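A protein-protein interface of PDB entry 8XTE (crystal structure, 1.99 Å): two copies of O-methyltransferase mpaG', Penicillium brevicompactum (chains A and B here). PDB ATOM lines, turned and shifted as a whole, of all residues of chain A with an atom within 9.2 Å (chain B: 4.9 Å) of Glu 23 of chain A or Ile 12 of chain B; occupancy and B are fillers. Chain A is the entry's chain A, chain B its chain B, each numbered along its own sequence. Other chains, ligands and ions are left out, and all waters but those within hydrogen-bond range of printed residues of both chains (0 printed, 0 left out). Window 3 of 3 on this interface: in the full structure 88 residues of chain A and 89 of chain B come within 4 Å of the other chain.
Along chain B the printed residues that touch a printed residue of chain A span positions 8 to 40.
Of the 19 printed residues of chain A, 6 touch a printed residue of chain B.
Printed residues of chain A that touch a printed residue of chain B: Leu 15, Ala 19, Tyr 22, Glu 23, Leu 33 and Ser 37.
Hydrophobic or aromatic side chains of chain A that line the printed part of chain B: Leu 15, Ala 19, Tyr 22 and Leu 33.
Of the printed residues of chain B, Ala 19 of chain A touches Ile 12.
Of the printed residues of chain B, Tyr 22 of chain A touches Pro 8 (3.9 Å).
Of chain B, only Ile 12 (3.8 Å) comes within 4 Å of Glu 23 of chain A.
Of the printed residues of chain B, Leu 33 of chain A touches Ile 12 (3.9 Å) and Leu 40 (3.9 Å).
Printed residues of chain B within 4 Å of Ser 37 of chain A: Leu 40.
Of chain A, only Ala 19, Glu 23 and Leu 33 come within 4 Å of Ile 12 of chain B.
Printed residues of chain A within 4 Å of Leu 15 of chain B: Leu 15 (3.7 Å).
The side-chain hydroxyl (OG) of Ser 37 of chain A sits at hydrogen-bond distance from the backbone carbonyl oxygen (O) of Leu 33 of chain A (2.8 Å).
Among the printed residues, merely in contact across the chains: Leu 15 of chain A with Leu 15 of chain B, Ala 19 of chain A with Ile 12 of chain B, Tyr 22 of chain A with Pro 8 of chain B, Glu 23 of chain A with Ile 12 of chain B, Leu 33 of chain A with Ile 12 of chain B, Leu 33 of chain A with Leu 40 of chain B and Ser 37 of chain A with Leu 40 of chain B.
Leu 15 of chain B touches its own counterpart, Leu 15 of chain A.
Of the 7 pairs that touch across the chains among the printed residues, 1 has its exchanged pair printed and touching as well.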
ATOM      1  N   ILE A  12      -3.458 -13.180 -30.599  1.00  0.00           N
ATOM      2  CA  ILE A  12      -3.190 -11.852 -31.145  1.00  0.00           C
ATOM      3  C   ILE A  12      -4.253 -10.860 -30.688  1.00  0.00           C
ATOM      4  O   ILE A  12      -3.943  -9.712 -30.342  1.00  0.00           O
ATOM      5  CB  ILE A  12      -3.089 -11.928 -32.683  1.00  0.00           C
ATOM      6  CG1 ILE A  12      -1.685 -12.379 -33.103  1.00  0.00           C
ATOM      7  CG2 ILE A  12      -3.449 -10.598 -33.329  1.00  0.00           C
ATOM      8  CD1 ILE A  12      -1.590 -12.853 -34.534  1.00  0.00           C
ATOM      9  N   LEU A  15      -4.010 -10.319 -26.752  1.00  0.00           N
ATOM     10  CA  LEU A  15      -2.868  -9.437 -26.529  1.00  0.00           C
ATOM     11  C   LEU A  15      -3.220  -7.992 -26.865  1.00  0.00           C
ATOM     12  O   LEU A  15      -2.833  -7.066 -26.140  1.00  0.00           O
ATOM     13  CB  LEU A  15      -1.673  -9.917 -27.357  1.00  0.00           C
ATOM     14  CG  LEU A  15      -0.272  -9.342 -27.140  1.00  0.00           C
ATOM     15  CD1 LEU A  15       0.780 -10.366 -27.558  1.00  0.00           C
ATOM     16  CD2 LEU A  15      -0.079  -8.043 -27.916  1.00  0.00           C
ATOM     17  N   ALA A  16      -3.961  -7.778 -27.958  1.00  0.00           N
ATOM     18  CA  ALA A  16      -4.384  -6.425 -28.308  1.00  0.00           C
ATOM     19  C   ALA A  16      -5.415  -5.896 -27.319  1.00  0.00           C
ATOM     20  O   ALA A  16      -5.414  -4.702 -26.993  1.00  0.00           O
ATOM     21  CB  ALA A  16      -4.939  -6.397 -29.733  1.00  0.00           C
ATOM     22  N   SER A  17      -6.301  -6.765 -26.828  1.00  0.00           N
ATOM     23  CA  SER A  17      -7.278  -6.341 -25.830  1.00  0.00           C
ATOM     24  C   SER A  17      -6.591  -5.941 -24.529  1.00  0.00           C
ATOM     25  O   SER A  17      -6.852  -4.861 -23.984  1.00  0.00           O
ATOM     26  CB  SER A  17      -8.298  -7.455 -25.586  1.00  0.00           C
ATOM     27  OG  SER A  17      -8.922  -7.313 -24.320  1.00  0.00           O
ATOM     28  N   ALA A  18      -5.702  -6.800 -24.019  1.00  0.00           N
ATOM     29  CA  ALA A  18      -4.973  -6.467 -22.800  1.00  0.00           C
ATOM     30  C   ALA A  18      -4.073  -5.254 -22.999  1.00  0.00           C
ATOM     31  O   ALA A  18      -3.763  -4.549 -22.032  1.00  0.00           O
ATOM     32  CB  ALA A  18      -4.154  -7.668 -22.329  1.00  0.00           C
ATOM     33  N   ALA A  19      -3.646  -4.994 -24.239  1.00  0.00           N
ATOM     34  CA  ALA A  19      -2.878  -3.785 -24.519  1.00  0.00           C
ATOM     35  C   ALA A  19      -3.711  -2.535 -24.260  1.00  0.00           C
ATOM     36  O   ALA A  19      -3.224  -1.571 -23.656  1.00  0.00           O
ATOM     37  CB  ALA A  19      -2.370  -3.802 -25.959  1.00  0.00           C
ATOM     38  N   LYS A  20      -4.968  -2.534 -24.711  1.00  0.00           N
ATOM     39  CA  LYS A  20      -5.870  -1.427 -24.411  1.00  0.00           C
ATOM     40  C   LYS A  20      -6.038  -1.254 -22.908  1.00  0.00           C
ATOM     41  O   LYS A  20      -5.999  -0.132 -22.389  1.00  0.00           O
ATOM     42  CB  LYS A  20      -7.228  -1.661 -25.073  1.00  0.00           C
ATOM     43  CG  LYS A  20      -8.099  -0.413 -25.163  1.00  0.00           C
ATOM     44  CD  LYS A  20      -9.411  -0.670 -25.902  1.00  0.00           C
ATOM     45  CE  LYS A  20      -9.376  -1.957 -26.719  1.00  0.00           C
ATOM     46  NZ  LYS A  20     -10.706  -2.274 -27.315  1.00  0.00           N
ATOM     47  N   GLN A  21      -6.232  -2.364 -22.192  1.00  0.00           N
ATOM     48  CA  GLN A  21      -6.377  -2.300 -20.742  1.00  0.00           C
ATOM     49  C   GLN A  21      -5.108  -1.769 -20.082  1.00  0.00           C
ATOM     50  O   GLN A  21      -5.177  -1.023 -19.098  1.00  0.00           O
ATOM     51  CB  GLN A  21      -6.732  -3.686 -20.206  1.00  0.00           C
ATOM     52  CG  GLN A  21      -7.892  -4.343 -20.943  1.00  0.00           C
ATOM     53  CD  GLN A  21      -8.053  -5.810 -20.596  1.00  0.00           C
ATOM     54  OE1 GLN A  21      -8.207  -6.656 -21.479  1.00  0.00           O
ATOM     55  NE2 GLN A  21      -8.016  -6.122 -19.305  1.00  0.00           N
ATOM     56  N   TYR A  22      -3.939  -2.139 -20.617  1.00  0.00           N
ATOM     57  CA  TYR A  22      -2.678  -1.647 -20.070  1.00  0.00           C
ATOM     58  C   TYR A  22      -2.529  -0.148 -20.285  1.00  0.00           C
ATOM     59  O   TYR A  22      -2.027   0.566 -19.409  1.00  0.00           O
ATOM     60  CB  TYR A  22      -1.508  -2.400 -20.704  1.00  0.00           C
ATOM     61  CG  TYR A  22      -0.155  -1.764 -20.476  1.00  0.00           C
ATOM     62  CD1 TYR A  22       0.458  -1.814 -19.229  1.00  0.00           C
ATOM     63  CD2 TYR A  22       0.515  -1.120 -21.509  1.00  0.00           C
ATOM     64  CE1 TYR A  22       1.695  -1.238 -19.017  1.00  0.00           C
ATOM     65  CE2 TYR A  22       1.753  -0.540 -21.304  1.00  0.00           C
ATOM     66  CZ  TYR A  22       2.337  -0.603 -20.056  1.00  0.00           C
ATOM     67  OH  TYR A  22       3.569  -0.031 -19.843  1.00  0.00           O
ATOM     68  N   GLU A  23      -2.963   0.345 -21.441  1.00  0.00           N
ATOM     69  CA  GLU A  23      -2.833   1.760 -21.753  1.00  0.00           C
ATOM     70  C   GLU A  23      -3.857   2.611 -21.010  1.00  0.00           C
ATOM     71  O   GLU A  23      -3.687   3.832 -20.927  1.00  0.00           O
ATOM     72  CB  GLU A  23      -2.934   1.941 -23.268  1.00  0.00           C
ATOM     73  CG  GLU A  23      -1.644   1.521 -23.979  1.00  0.00           C
ATOM     74  CD  GLU A  23      -1.857   1.067 -25.413  1.00  0.00           C
ATOM     75  OE1 GLU A  23      -3.009   0.749 -25.778  1.00  0.00           O
ATOM     76  OE2 GLU A  23      -0.862   1.004 -26.171  1.00  0.00           O
ATOM     77  N   ASN A  24      -4.901   1.991 -20.460  1.00  0.00           N
ATOM     78  CA  ASN A  24      -5.827   2.638 -19.539  1.00  0.00           C
ATOM     79  C   ASN A  24      -5.383   2.533 -18.086  1.00  0.00           C
ATOM     80  O   ASN A  24      -6.106   2.997 -17.199  1.00  0.00           O
ATOM     81  CB  ASN A  24      -7.228   2.032 -19.680  1.00  0.00           C
ATOM     82  CG  ASN A  24      -8.327   3.010 -19.311  1.00  0.00           C
ATOM     83  OD1 ASN A  24      -8.146   4.226 -19.401  1.00  0.00           O
ATOM     84  ND2 ASN A  24      -9.466   2.485 -18.876  1.00  0.00           N
ATOM     85  N   ASN A  25      -4.224   1.921 -17.829  1.00  0.00           N
ATOM     86  CA  ASN A  25      -3.688   1.745 -16.477  1.00  0.00           C
ATOM     87  C   ASN A  25      -4.653   0.954 -15.594  1.00  0.00           C
ATOM     88  O   ASN A  25      -4.971   1.346 -14.469  1.00  0.00           O
ATOM     89  CB  ASN A  25      -3.339   3.094 -15.840  1.00  0.00           C
ATOM     90  CG  ASN A  25      -1.886   3.477 -16.049  1.00  0.00           C
ATOM     91  OD1 ASN A  25      -1.200   3.878 -15.109  1.00  0.00           O
ATOM     92  ND2 ASN A  25      -1.409   3.351 -17.283  1.00  0.00           N
ATOM     93  N   GLU A  26      -5.118  -0.178 -16.116  1.00  0.00           N
ATOM     94  CA  GLU A  26      -5.994  -1.065 -15.368  1.00  0.00           C
ATOM     95  C   GLU A  26      -5.166  -2.033 -14.531  1.00  0.00           C
ATOM     96  O   GLU A  26      -4.063  -2.434 -14.918  1.00  0.00           O
ATOM     97  CB  GLU A  26      -6.923  -1.829 -16.313  1.00  0.00           C
ATOM     98  CG  GLU A  26      -7.808  -0.911 -17.151  1.00  0.00           C
ATOM     99  CD  GLU A  26      -8.864  -1.659 -17.941  1.00  0.00           C
ATOM    100  OE1 GLU A  26      -9.010  -2.882 -17.735  1.00  0.00           O
ATOM    101  OE2 GLU A  26      -9.547  -1.021 -18.773  1.00  0.00           O
ATOM    102  N   SER A  27      -5.708  -2.395 -13.369  1.00  0.00           N
ATOM    103  CA  SER A  27      -4.967  -3.202 -12.405  1.00  0.00           C
ATOM    104  C   SER A  27      -4.586  -4.553 -13.000  1.00  0.00           C
ATOM    105  O   SER A  27      -5.436  -5.276 -13.528  1.00  0.00           O
ATOM    106  CB  SER A  27      -5.804  -3.403 -11.142  1.00  0.00           C
ATOM    107  OG  SER A  27      -5.620  -2.334 -10.231  1.00  0.00           O
ATOM    108  N   ALA A  29      -2.964  -5.161 -15.654  1.00  0.00           N
ATOM    109  CA  ALA A  29      -2.928  -5.218 -17.111  1.00  0.00           C
ATOM    110  C   ALA A  29      -1.504  -5.336 -17.641  1.00  0.00           C
ATOM    111  O   ALA A  29      -1.291  -5.931 -18.704  1.00  0.00           O
ATOM    112  CB  ALA A  29      -3.616  -3.990 -17.699  1.00  0.00           C
ATOM    113  N   ARG A  30      -0.525  -4.772 -16.929  1.00  0.00           N
ATOM    114  CA  ARG A  30       0.872  -4.988 -17.294  1.00  0.00           C
ATOM    115  C   ARG A  30       1.223  -6.467 -17.230  1.00  0.00           C
ATOM    116  O   ARG A  30       1.853  -7.014 -18.142  1.00  0.00           O
ATOM    117  CB  ARG A  30       1.783  -4.182 -16.367  1.00  0.00           C
ATOM    118  CG  ARG A  30       3.245  -4.139 -16.791  1.00  0.00           C
ATOM    119  CD  ARG A  30       4.078  -3.408 -15.744  1.00  0.00           C
ATOM    120  NE  ARG A  30       4.109  -4.128 -14.475  1.00  0.00           N
ATOM    121  CZ  ARG A  30       4.756  -5.269 -14.273  1.00  0.00           C
ATOM    122  NH1 ARG A  30       5.503  -5.818 -15.214  1.00  0.00           N
ATOM    123  NH2 ARG A  30       4.657  -5.869 -13.089  1.00  0.00           N
ATOM    124  N   LEU A  33      -0.392  -8.571 -20.024  1.00  0.00           N
ATOM    125  CA  LEU A  33       0.192  -8.398 -21.350  1.00  0.00           C
ATOM    126  C   LEU A  33       1.450  -9.245 -21.507  1.00  0.00           C
ATOM    127  O   LEU A  33       1.668  -9.847 -22.565  1.00  0.00           O
ATOM    128  CB  LEU A  33       0.490  -6.922 -21.606  1.00  0.00           C
ATOM    129  CG  LEU A  33       0.852  -6.531 -23.041  1.00  0.00           C
ATOM    130  CD1 LEU A  33      -0.022  -7.263 -24.042  1.00  0.00           C
ATOM    131  CD2 LEU A  33       0.730  -5.028 -23.228  1.00  0.00           C
ATOM    132  N   ILE A  34       2.284  -9.311 -20.465  1.00  0.00           N
ATOM    133  CA  ILE A  34       3.418 -10.232 -20.477  1.00  0.00           C
ATOM    134  C   ILE A  34       2.934 -11.665 -20.657  1.00  0.00           C
ATOM    135  O   ILE A  34       3.516 -12.443 -21.425  1.00  0.00           O
ATOM    136  CB  ILE A  34       4.252 -10.075 -19.192  1.00  0.00           C
ATOM    137  CG1 ILE A  34       5.008  -8.742 -19.197  1.00  0.00           C
ATOM    138  CG2 ILE A  34       5.226 -11.238 -19.027  1.00  0.00           C
ATOM    139  CD1 ILE A  34       5.386  -8.254 -17.819  1.00  0.00           C
ATOM    140  N   SER A  37       1.849 -12.269 -24.128  1.00  0.00           N
ATOM    141  CA  SER A  37       3.033 -12.296 -24.983  1.00  0.00           C
ATOM    142  C   SER A  37       3.738 -13.643 -24.904  1.00  0.00           C
ATOM    143  O   SER A  37       4.193 -14.173 -25.924  1.00  0.00           O
ATOM    144  CB  SER A  37       3.992 -11.173 -24.590  1.00  0.00           C
ATOM    145  OG  SER A  37       3.403  -9.906 -24.819  1.00  0.00           O
ATOM    146  N   PRO B   8       6.727   0.634 -24.677  1.00  0.00           N
ATOM    147  CA  PRO B   8       5.729  -0.439 -24.816  1.00  0.00           C
ATOM    148  C   PRO B   8       4.636  -0.123 -25.825  1.00  0.00           C
ATOM    149  O   PRO B   8       4.202  -1.018 -26.561  1.00  0.00           O
ATOM    150  CB  PRO B   8       5.186  -0.558 -23.389  1.00  0.00           C
ATOM    151  CG  PRO B   8       6.414  -0.327 -22.568  1.00  0.00           C
ATOM    152  CD  PRO B   8       7.045   0.875 -23.256  1.00  0.00           C
ATOM    153  N   ALA B   9       4.180   1.133 -25.884  1.00  0.00           N
ATOM    154  CA  ALA B   9       3.180   1.508 -26.878  1.00  0.00           C
ATOM    155  C   ALA B   9       3.729   1.366 -28.293  1.00  0.00           C
ATOM    156  O   ALA B   9       3.001   0.974 -29.215  1.00  0.00           O
ATOM    157  CB  ALA B   9       2.701   2.940 -26.630  1.00  0.00           C
ATOM    158  N   SER B  10       5.014   1.673 -28.484  1.00  0.00           N
ATOM    159  CA  SER B  10       5.631   1.520 -29.796  1.00  0.00           C
ATOM    160  C   SER B  10       5.761   0.048 -30.185  1.00  0.00           C
ATOM    161  O   SER B  10       5.536  -0.313 -31.348  1.00  0.00           O
ATOM    162  CB  SER B  10       6.995   2.214 -29.808  1.00  0.00           C
ATOM    163  OG  SER B  10       7.919   1.537 -30.643  1.00  0.00           O
ATOM    164  N   ILE B  11       6.120  -0.817 -29.231  1.00  0.00           N
ATOM    165  CA  ILE B  11       6.255  -2.241 -29.529  1.00  0.00           C
ATOM    166  C   ILE B  11       4.890  -2.869 -29.792  1.00  0.00           C
ATOM    167  O   ILE B  11       4.749  -3.728 -30.671  1.00  0.00           O
ATOM    168  CB  ILE B  11       7.002  -2.961 -28.389  1.00  0.00           C
ATOM    169  CG1 ILE B  11       8.419  -2.405 -28.242  1.00  0.00           C
ATOM    170  CG2 ILE B  11       7.042  -4.466 -28.629  1.00  0.00           C
ATOM    171  CD1 ILE B  11       8.941  -2.449 -26.830  1.00  0.00           C
ATOM    172  N   ILE B  12       3.866  -2.451 -29.040  1.00  0.00           N
ATOM    173  CA  ILE B  12       2.515  -2.971 -29.248  1.00  0.00           C
ATOM    174  C   ILE B  12       2.065  -2.730 -30.685  1.00  0.00           C
ATOM    175  O   ILE B  12       1.417  -3.586 -31.300  1.00  0.00           O
ATOM    176  CB  ILE B  12       1.540  -2.350 -28.226  1.00  0.00           C
ATOM    177  CG1 ILE B  12       1.729  -2.980 -26.843  1.00  0.00           C
ATOM    178  CG2 ILE B  12       0.097  -2.513 -28.674  1.00  0.00           C
ATOM    179  CD1 ILE B  12       1.211  -2.118 -25.707  1.00  0.00           C
ATOM    180  N   GLN B  13       2.419  -1.570 -31.250  1.00  0.00           N
ATOM    181  CA  GLN B  13       2.109  -1.302 -32.654  1.00  0.00           C
ATOM    182  C   GLN B  13       2.928  -2.189 -33.586  1.00  0.00           C
ATOM    183  O   GLN B  13       2.395  -2.726 -34.565  1.00  0.00           O
ATOM    184  CB  GLN B  13       2.356   0.169 -32.985  1.00  0.00           C
ATOM    185  CG  GLN B  13       1.438   1.155 -32.291  1.00  0.00           C
ATOM    186  CD  GLN B  13       1.655   2.578 -32.778  1.00  0.00           C
ATOM    187  OE1 GLN B  13       1.496   2.873 -33.966  1.00  0.00           O
ATOM    188  NE2 GLN B  13       2.023   3.469 -31.862  1.00  0.00           N
ATOM    189  N   GLU B  14       4.228  -2.338 -33.313  1.00  0.00           N
ATOM    190  CA  GLU B  14       5.071  -3.146 -34.189  1.00  0.00           C
ATOM    191  C   GLU B  14       4.710  -4.620 -34.107  1.00  0.00           C
ATOM    192  O   GLU B  14       4.909  -5.364 -35.076  1.00  0.00           O
ATOM    193  CB  GLU B  14       6.545  -2.933 -33.845  1.00  0.00           C
ATOM    194  CG  GLU B  14       7.063  -1.516 -34.099  1.00  0.00           C
ATOM    195  CD  GLU B  14       7.195  -1.161 -35.579  1.00  0.00           C
ATOM    196  OE1 GLU B  14       6.313  -1.523 -36.388  1.00  0.00           O
ATOM    197  OE2 GLU B  14       8.199  -0.506 -35.935  1.00  0.00           O
ATOM    198  N   LEU B  15       4.183  -5.063 -32.967  1.00  0.00           N
ATOM    199  CA  LEU B  15       3.659  -6.420 -32.879  1.00  0.00           C
ATOM    200  C   LEU B  15       2.397  -6.568 -33.724  1.00  0.00           C
ATOM    201  O   LEU B  15       2.254  -7.543 -34.472  1.00  0.00           O
ATOM    202  CB  LEU B  15       3.392  -6.766 -31.414  1.00  0.00           C
ATOM    203  CG  LEU B  15       3.166  -8.218 -31.008  1.00  0.00           C
ATOM    204  CD1 LEU B  15       3.669  -8.416 -29.595  1.00  0.00           C
ATOM    205  CD2 LEU B  15       1.690  -8.591 -31.110  1.00  0.00           C
ATOM    206  N   ALA B  16       1.484  -5.596 -33.632  1.00  0.00           N
ATOM    207  CA  ALA B  16       0.256  -5.647 -34.417  1.00  0.00           C
ATOM    208  C   ALA B  16       0.537  -5.605 -35.914  1.00  0.00           C
ATOM    209  O   ALA B  16      -0.215  -6.195 -36.699  1.00  0.00           O
ATOM    210  CB  ALA B  16      -0.668  -4.496 -34.021  1.00  0.00           C
ATOM    211  N   LEU B  40       8.435  -6.966 -26.205  1.00  0.00           N
ATOM    212  CA  LEU B  40       7.361  -6.407 -25.388  1.00  0.00           C
ATOM    213  C   LEU B  40       7.470  -6.876 -23.943  1.00  0.00           C
ATOM    214  O   LEU B  40       7.215  -6.102 -23.014  1.00  0.00           O
ATOM    215  CB  LEU B  40       5.994  -6.783 -25.966  1.00  0.00           C
ATOM    216  CG  LEU B  40       4.773  -6.162 -25.264  1.00  0.00           C
ATOM    217  CD1 LEU B  40       4.915  -4.647 -25.155  1.00  0.00           C
ATOM    218  CD2 LEU B  40       3.474  -6.533 -25.966  1.00  0.00           C
